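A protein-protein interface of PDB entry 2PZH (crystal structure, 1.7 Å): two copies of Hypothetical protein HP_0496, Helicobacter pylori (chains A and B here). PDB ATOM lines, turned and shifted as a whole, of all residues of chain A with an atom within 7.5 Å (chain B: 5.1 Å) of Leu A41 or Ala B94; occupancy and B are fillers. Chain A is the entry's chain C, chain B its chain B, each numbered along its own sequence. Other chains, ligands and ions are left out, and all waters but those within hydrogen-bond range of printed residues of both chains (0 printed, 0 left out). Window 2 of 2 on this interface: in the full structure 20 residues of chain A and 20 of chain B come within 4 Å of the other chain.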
ATOM      1  N   SER A  32       5.385  15.358  -8.243  1.00  0.00           N
ATOM      2  CA  SER A  32       6.143  14.405  -7.440  1.00  0.00           C
ATOM      3  C   SER A  32       5.676  14.441  -5.981  1.00  0.00           C
ATOM      4  O   SER A  32       5.633  13.418  -5.308  1.00  0.00           O
ATOM      5  CB  SER A  32       7.649  14.683  -7.529  1.00  0.00           C
ATOM      6  OG  SER A  32       8.168  14.226  -8.771  1.00  0.00           O
ATOM      7  N   PHE A  35       3.084  12.005  -5.050  1.00  0.00           N
ATOM      8  CA  PHE A  35       3.618  10.667  -4.814  1.00  0.00           C
ATOM      9  C   PHE A  35       4.345  10.615  -3.479  1.00  0.00           C
ATOM     10  O   PHE A  35       4.117   9.709  -2.699  1.00  0.00           O
ATOM     11  CB  PHE A  35       4.522  10.196  -5.953  1.00  0.00           C
ATOM     12  CG  PHE A  35       3.787   9.928  -7.243  1.00  0.00           C
ATOM     13  CD1 PHE A  35       3.509   8.632  -7.642  1.00  0.00           C
ATOM     14  CD2 PHE A  35       3.382  10.974  -8.060  1.00  0.00           C
ATOM     15  CE1 PHE A  35       2.838   8.386  -8.837  1.00  0.00           C
ATOM     16  CE2 PHE A  35       2.716  10.743  -9.257  1.00  0.00           C
ATOM     17  CZ  PHE A  35       2.436   9.443  -9.642  1.00  0.00           C
ATOM     18  N   PHE A  36       5.215  11.589  -3.213  1.00  0.00           N
ATOM     19  CA  PHE A  36       5.967  11.615  -1.959  1.00  0.00           C
ATOM     20  C   PHE A  36       5.037  11.619  -0.740  1.00  0.00           C
ATOM     21  O   PHE A  36       5.372  11.050   0.299  1.00  0.00           O
ATOM     22  CB  PHE A  36       6.889  12.841  -1.866  1.00  0.00           C
ATOM     23  CG  PHE A  36       7.972  12.891  -2.911  1.00  0.00           C
ATOM     24  CD1 PHE A  36       8.496  11.739  -3.467  1.00  0.00           C
ATOM     25  CD2 PHE A  36       8.483  14.117  -3.322  1.00  0.00           C
ATOM     26  CE1 PHE A  36       9.508  11.814  -4.432  1.00  0.00           C
ATOM     27  CE2 PHE A  36       9.478  14.194  -4.282  1.00  0.00           C
ATOM     28  CZ  PHE A  36       9.994  13.047  -4.829  1.00  0.00           C
ATOM     29  N   LYS A  37       3.889  12.278  -0.855  1.00  0.00           N
ATOM     30  CA  LYS A  37       2.933  12.311   0.255  1.00  0.00           C
ATOM     31  C   LYS A  37       2.333  10.936   0.570  1.00  0.00           C
ATOM     32  O   LYS A  37       2.045  10.626   1.734  1.00  0.00           O
ATOM     33  CB  LYS A  37       1.816  13.314  -0.008  1.00  0.00           C
ATOM     34  CG  LYS A  37       2.223  14.761   0.120  1.00  0.00           C
ATOM     35  CD  LYS A  37       0.973  15.629   0.133  1.00  0.00           C
ATOM     36  CE  LYS A  37       1.244  17.002  -0.448  1.00  0.00           C
ATOM     37  NZ  LYS A  37       0.009  17.842  -0.452  1.00  0.00           N
ATOM     38  N   GLN A  38       2.141  10.116  -0.457  1.00  0.00           N
ATOM     39  CA  GLN A  38       1.714   8.729  -0.250  1.00  0.00           C
ATOM     40  C   GLN A  38       2.910   7.833   0.033  1.00  0.00           C
ATOM     41  O   GLN A  38       2.823   6.603  -0.105  1.00  0.00           O
ATOM     42  CB  GLN A  38       0.937   8.193  -1.454  1.00  0.00           C
ATOM     43  CG  GLN A  38      -0.583   8.168  -1.278  1.00  0.00           C
ATOM     44  CD  GLN A  38      -1.217   9.493  -1.629  1.00  0.00           C
ATOM     45  OE1 GLN A  38      -0.946  10.054  -2.697  1.00  0.00           O
ATOM     46  NE2 GLN A  38      -2.062  10.007  -0.738  1.00  0.00           N
ATOM     47  N   ASN A  39       4.022   8.455   0.424  1.00  0.00           N
ATOM     48  CA  ASN A  39       5.251   7.742   0.799  1.00  0.00           C
ATOM     49  C   ASN A  39       5.891   6.930  -0.325  1.00  0.00           C
ATOM     50  O   ASN A  39       6.656   5.991  -0.076  1.00  0.00           O
ATOM     51  CB  ASN A  39       5.025   6.858   2.029  1.00  0.00           C
ATOM     52  CG  ASN A  39       4.342   7.604   3.170  1.00  0.00           C
ATOM     53  OD1 ASN A  39       3.398   7.091   3.775  1.00  0.00           O
ATOM     54  ND2 ASN A  39       4.803   8.820   3.456  1.00  0.00           N
ATOM     55  N   VAL A  40       5.594   7.287  -1.566  1.00  0.00           N
ATOM     56  CA  VAL A  40       6.210   6.580  -2.678  1.00  0.00           C
ATOM     57  C   VAL A  40       6.950   7.558  -3.579  1.00  0.00           C
ATOM     58  O   VAL A  40       6.677   8.755  -3.576  1.00  0.00           O
ATOM     59  CB  VAL A  40       5.177   5.749  -3.477  1.00  0.00           C
ATOM     60  CG1 VAL A  40       3.991   6.597  -3.871  1.00  0.00           C
ATOM     61  CG2 VAL A  40       5.819   5.117  -4.714  1.00  0.00           C
ATOM     62  N   LEU A  41       7.929   7.048  -4.312  1.00  0.00           N
ATOM     63  CA  LEU A  41       8.523   7.819  -5.369  1.00  0.00           C
ATOM     64  C   LEU A  41       7.677   7.517  -6.588  1.00  0.00           C
ATOM     65  O   LEU A  41       7.039   6.450  -6.657  1.00  0.00           O
ATOM     66  CB  LEU A  41       9.987   7.413  -5.576  1.00  0.00           C
ATOM     67  CG  LEU A  41      10.827   7.309  -4.292  1.00  0.00           C
ATOM     68  CD1 LEU A  41      12.135   6.577  -4.557  1.00  0.00           C
ATOM     69  CD2 LEU A  41      11.085   8.677  -3.646  1.00  0.00           C
ATOM     70  N   PRO A  42       7.621   8.459  -7.540  1.00  0.00           N
ATOM     71  CA  PRO A  42       6.890   8.232  -8.789  1.00  0.00           C
ATOM     72  C   PRO A  42       7.612   7.291  -9.761  1.00  0.00           C
ATOM     73  O   PRO A  42       7.682   7.566 -10.960  1.00  0.00           O
ATOM     74  CB  PRO A  42       6.779   9.639  -9.390  1.00  0.00           C
ATOM     75  CG  PRO A  42       7.919  10.382  -8.833  1.00  0.00           C
ATOM     76  CD  PRO A  42       8.208   9.810  -7.473  1.00  0.00           C
ATOM     77  N   GLU A  43       8.125   6.184  -9.239  1.00  0.00           N
ATOM     78  CA  GLU A  43       8.808   5.180 -10.042  1.00  0.00           C
ATOM     79  C   GLU A  43       8.854   3.903  -9.216  1.00  0.00           C
ATOM     80  O   GLU A  43       8.737   3.953  -7.986  1.00  0.00           O
ATOM     81  CB  GLU A  43      10.234   5.640 -10.362  1.00  0.00           C
ATOM     82  CG  GLU A  43      10.880   6.415  -9.207  1.00  0.00           C
ATOM     83  CD  GLU A  43      12.387   6.564  -9.340  1.00  0.00           C
ATOM     84  OE1 GLU A  43      13.108   5.558  -9.160  1.00  0.00           O
ATOM     85  OE2 GLU A  43      12.849   7.696  -9.602  1.00  0.00           O
ATOM     86  N   ASN A  44       9.031   2.767  -9.881  1.00  0.00           N
ATOM     87  CA  ASN A  44       9.199   1.505  -9.167  1.00  0.00           C
ATOM     88  C   ASN A  44      10.300   0.616  -9.753  1.00  0.00           C
ATOM     89  O   ASN A  44      11.089   1.071 -10.584  1.00  0.00           O
ATOM     90  CB  ASN A  44       7.860   0.763  -8.983  1.00  0.00           C
ATOM     91  CG  ASN A  44       7.187   0.402 -10.297  1.00  0.00           C
ATOM     92  OD1 ASN A  44       7.814   0.370 -11.357  1.00  0.00           O
ATOM     93  ND2 ASN A  44       5.898   0.097 -10.222  1.00  0.00           N
ATOM     94  N   GLY A  47      10.004   0.487 -13.685  1.00  0.00           N
ATOM     95  CA  GLY A  47       9.203   1.446 -14.428  1.00  0.00           C
ATOM     96  C   GLY A  47       9.384   2.872 -13.965  1.00  0.00           C
ATOM     97  O   GLY A  47       9.531   3.140 -12.771  1.00  0.00           O
ATOM     98  N   PHE A  49       7.976   7.112 -15.047  1.00  0.00           N
ATOM     99  CA  PHE A  49       7.126   7.972 -15.862  1.00  0.00           C
ATOM    100  C   PHE A  49       7.996   8.767 -16.812  1.00  0.00           C
ATOM    101  O   PHE A  49       9.038   9.295 -16.412  1.00  0.00           O
ATOM    102  CB  PHE A  49       6.301   8.930 -14.994  1.00  0.00           C
ATOM    103  CG  PHE A  49       5.106   8.288 -14.361  1.00  0.00           C
ATOM    104  CD1 PHE A  49       3.969   8.029 -15.113  1.00  0.00           C
ATOM    105  CD2 PHE A  49       5.122   7.925 -13.022  1.00  0.00           C
ATOM    106  CE1 PHE A  49       2.859   7.417 -14.535  1.00  0.00           C
ATOM    107  CE2 PHE A  49       4.010   7.312 -12.441  1.00  0.00           C
ATOM    108  CZ  PHE A  49       2.882   7.062 -13.205  1.00  0.00           C
ATOM    109  N   PHE A 113       4.241   5.663 -19.033  1.00  0.00           N
ATOM    110  CA  PHE A 113       5.030   4.912 -18.051  1.00  0.00           C
ATOM    111  C   PHE A 113       5.857   3.884 -18.821  1.00  0.00           C
ATOM    112  O   PHE A 113       5.328   3.184 -19.686  1.00  0.00           O
ATOM    113  CB  PHE A 113       4.115   4.221 -17.019  1.00  0.00           C
ATOM    114  CG  PHE A 113       4.827   3.774 -15.765  1.00  0.00           C
ATOM    115  CD1 PHE A 113       5.183   4.691 -14.786  1.00  0.00           C
ATOM    116  CD2 PHE A 113       5.144   2.437 -15.565  1.00  0.00           C
ATOM    117  CE1 PHE A 113       5.845   4.286 -13.627  1.00  0.00           C
ATOM    118  CE2 PHE A 113       5.807   2.029 -14.418  1.00  0.00           C
ATOM    119  CZ  PHE A 113       6.156   2.961 -13.442  1.00  0.00           C
ATOM    120  N   PHE A 128      -0.042   3.400  -8.599  1.00  0.00           N
ATOM    121  CA  PHE A 128       0.080   4.726  -9.211  1.00  0.00           C
ATOM    122  C   PHE A 128      -1.215   5.150  -9.917  1.00  0.00           C
ATOM    123  O   PHE A 128      -1.563   6.332  -9.940  1.00  0.00           O
ATOM    124  CB  PHE A 128       1.278   4.789 -10.179  1.00  0.00           C
ATOM    125  CG  PHE A 128       2.623   4.585  -9.516  1.00  0.00           C
ATOM    126  CD1 PHE A 128       2.777   4.720  -8.139  1.00  0.00           C
ATOM    127  CD2 PHE A 128       3.753   4.298 -10.279  1.00  0.00           C
ATOM    128  CE1 PHE A 128       4.021   4.541  -7.537  1.00  0.00           C
ATOM    129  CE2 PHE A 128       5.002   4.112  -9.680  1.00  0.00           C
ATOM    130  CZ  PHE A 128       5.135   4.233  -8.308  1.00  0.00           C
ATOM    131  N   LEU A 131      -3.505   6.348  -7.207  1.00  0.00           N
ATOM    132  CA  LEU A 131      -2.964   7.626  -6.758  1.00  0.00           C
ATOM    133  C   LEU A 131      -3.383   8.729  -7.719  1.00  0.00           C
ATOM    134  O   LEU A 131      -3.890   9.774  -7.308  1.00  0.00           O
ATOM    135  CB  LEU A 131      -1.432   7.582  -6.682  1.00  0.00           C
ATOM    136  CG  LEU A 131      -0.768   7.321  -5.330  1.00  0.00           C
ATOM    137  CD1 LEU A 131      -0.498   5.838  -5.120  1.00  0.00           C
ATOM    138  CD2 LEU A 131       0.527   8.098  -5.216  1.00  0.00           C
ATOM    139  N   ARG B   6      12.203  19.809   0.186  1.00  0.00           N
ATOM    140  CA  ARG B   6      12.147  18.471  -0.371  1.00  0.00           C
ATOM    141  C   ARG B   6      13.110  18.429  -1.551  1.00  0.00           C
ATOM    142  O   ARG B   6      13.162  19.389  -2.326  1.00  0.00           O
ATOM    143  CB  ARG B   6      10.726  18.236  -0.913  1.00  0.00           C
ATOM    144  CG  ARG B   6      10.518  16.897  -1.626  1.00  0.00           C
ATOM    145  CD  ARG B   6      10.291  15.754  -0.651  1.00  0.00           C
ATOM    146  NE  ARG B   6       8.924  15.735  -0.120  1.00  0.00           N
ATOM    147  CZ  ARG B   6       8.492  14.865   0.797  1.00  0.00           C
ATOM    148  NH1 ARG B   6       9.301  13.936   1.267  1.00  0.00           N
ATOM    149  NH2 ARG B   6       7.239  14.897   1.215  1.00  0.00           N
ATOM    150  N   LEU B  64      16.797  11.811  -3.812  1.00  0.00           N
ATOM    151  CA  LEU B  64      15.447  12.091  -4.257  1.00  0.00           C
ATOM    152  C   LEU B  64      14.431  11.850  -3.156  1.00  0.00           C
ATOM    153  O   LEU B  64      14.425  10.786  -2.540  1.00  0.00           O
ATOM    154  CB  LEU B  64      15.089  11.209  -5.457  1.00  0.00           C
ATOM    155  CG  LEU B  64      13.688  11.446  -6.018  1.00  0.00           C
ATOM    156  CD1 LEU B  64      13.597  12.817  -6.688  1.00  0.00           C
ATOM    157  CD2 LEU B  64      13.250  10.308  -6.993  1.00  0.00           C
ATOM    158  N   GLY B  65      13.569  12.836  -2.928  1.00  0.00           N
ATOM    159  CA  GLY B  65      12.397  12.663  -2.054  1.00  0.00           C
ATOM    160  C   GLY B  65      12.692  12.854  -0.575  1.00  0.00           C
ATOM    161  O   GLY B  65      11.787  12.824   0.258  1.00  0.00           O
ATOM    162  N   GLN B  66      13.960  13.058  -0.239  1.00  0.00           N
ATOM    163  CA  GLN B  66      14.305  13.334   1.147  1.00  0.00           C
ATOM    164  C   GLN B  66      13.876  14.732   1.567  1.00  0.00           C
ATOM    165  O   GLN B  66      13.758  15.622   0.745  1.00  0.00           O
ATOM    166  CB  GLN B  66      15.797  13.104   1.392  1.00  0.00           C
ATOM    167  CG  GLN B  66      16.137  11.631   1.371  1.00  0.00           C
ATOM    168  CD  GLN B  66      17.600  11.349   1.565  1.00  0.00           C
ATOM    169  OE1 GLN B  66      18.457  12.117   1.148  1.00  0.00           O
ATOM    170  NE2 GLN B  66      17.898  10.224   2.194  1.00  0.00           N
ATOM    171  N   GLN B  92      14.342  13.170   6.944  1.00  0.00           N
ATOM    172  CA  GLN B  92      13.282  12.231   6.594  1.00  0.00           C
ATOM    173  C   GLN B  92      13.468  11.686   5.178  1.00  0.00           C
ATOM    174  O   GLN B  92      13.938  12.396   4.295  1.00  0.00           O
ATOM    175  CB  GLN B  92      11.924  12.930   6.706  1.00  0.00           C
ATOM    176  CG  GLN B  92      10.716  12.013   6.788  1.00  0.00           C
ATOM    177  CD  GLN B  92       9.419  12.807   6.808  1.00  0.00           C
ATOM    178  OE1 GLN B  92       8.457  12.436   7.478  1.00  0.00           O
ATOM    179  NE2 GLN B  92       9.398  13.920   6.087  1.00  0.00           N
ATOM    180  N   ASN B  93      13.123  10.413   4.993  1.00  0.00           N
ATOM    181  CA  ASN B  93      12.995   9.782   3.679  1.00  0.00           C
ATOM    182  C   ASN B  93      11.573  10.032   3.175  1.00  0.00           C
ATOM    183  O   ASN B  93      10.675  10.276   3.980  1.00  0.00           O
ATOM    184  CB  ASN B  93      13.195   8.262   3.803  1.00  0.00           C
ATOM    185  CG  ASN B  93      14.633   7.869   4.091  1.00  0.00           C
ATOM    186  OD1 ASN B  93      14.921   7.168   5.069  1.00  0.00           O
ATOM    187  ND2 ASN B  93      15.541   8.308   3.235  1.00  0.00           N
ATOM    188  N   ALA B  94      11.341   9.944   1.868  1.00  0.00           N
ATOM    189  CA  ALA B  94       9.965  10.022   1.362  1.00  0.00           C
ATOM    190  C   ALA B  94       9.138   8.827   1.845  1.00  0.00           C
ATOM    191  O   ALA B  94       7.945   8.962   2.122  1.00  0.00           O
ATOM    192  CB  ALA B  94       9.938  10.093  -0.157  1.00  0.00           C
ATOM    193  N   SER B  95       9.791   7.670   1.931  1.00  0.00           N
ATOM    194  CA  SER B  95       9.187   6.401   2.372  1.00  0.00           C
ATOM    195  C   SER B  95       8.826   6.389   3.854  1.00  0.00           C
ATOM    196  O   SER B  95       8.080   5.509   4.309  1.00  0.00           O
ATOM    197  CB  SER B  95      10.179   5.267   2.139  1.00  0.00           C
ATOM    198  OG  SER B  95      11.232   5.381   3.084  1.00  0.00           O
ATOM    199  N   LEU B  96       9.409   7.317   4.610  1.00  0.00           N
ATOM    200  CA  LEU B  96       9.072   7.513   6.019  1.00  0.00           C
ATOM    201  C   LEU B  96       9.773   6.571   6.977  1.00  0.00           C
ATOM    202  O   LEU B  96       9.571   6.671   8.198  1.00  0.00           O
ATOM    203  CB  LEU B  96       7.561   7.381   6.245  1.00  0.00           C
ATOM    204  CG  LEU B  96       6.750   8.661   6.113  1.00  0.00           C
ATOM    205  CD1 LEU B  96       5.367   8.420   6.663  1.00  0.00           C
ATOM    206  CD2 LEU B  96       7.439   9.771   6.865  1.00  0.00           C
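The backbone carbonyl oxygen of Ala B94 sits close to the side-chain amide nitrogen of Asn A39, 3.4 Å away.
The backbone NH (N) of Ala B94 sits close to the backbone carbonyl oxygen (O) of Gly B65, 3.3 Å away. The guanidinium group of Arg B6 lies within hydrogen-bond range of the backbone carbonyl oxygen of Gly B65 (2.9 Å).
CD2 of Phe A36 touches NE of Arg B6, at 3.6 Å. Phe A36 touches Gly B65 (CZ to CA, 3.7 Å). Ala B94 touches Phe A36 (O to O, 3.8 Å). Ser B95 touches Asn A39 (CA to O, 3.5 Å). Leu B96 touches Asn A39. Ala B94 touches Leu A41. Leu B64 touches Glu A43 (CD2 to OE2, 3.7 Å).
Ser A32 touches none of the printed residues of chain B. Phe A35 touches none of the printed residues of chain B. Printed residues of chain B within 4 Å of Phe A36: Arg B6 (3.6 Å), Gly B65 (3.7 Å) and Ala B94 (3.8 Å). Printed residues of chain B within 4 Å of Asn A39: Ala B94, Ser B95 and Leu B96. Of chain B, only Ala B94 comes within 4 Å of Leu A41. Of the printed residues of chain B, Glu A43 touches Leu B64 (3.7 Å). Of the printed residues of chain A, Arg B6 touches Phe A36 (3.6 Å). Of the printed residues of chain A, Ala B94 touches Phe A36, Asn A39 and Leu A41. The nearest residue of chain A that does not touch Ala B94 is Val A40 (4.7 Å).
Of the 16 printed residues of chain A, 4 touch a printed residue of chain B. Hydrophobic or aromatic side chains of chain A within 4 Å of the printed part of chain B: Phe A36 and Leu A41. Along chain A the printed residues that touch a printed residue of chain B span positions 36 to 43. Of the 9 printed residues of chain B, 6 touch a printed residue of chain A. Hydrophobic or aromatic side chains of chain B within 4 Å of the printed part of chain A: Leu B64, Ala B94 and Leu B96. Along chain B the printed residues that touch a printed residue of chain A span positions 6 to 96. Among the printed residues, 8 pairs touch across the chains.
No position is printed for both chains.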
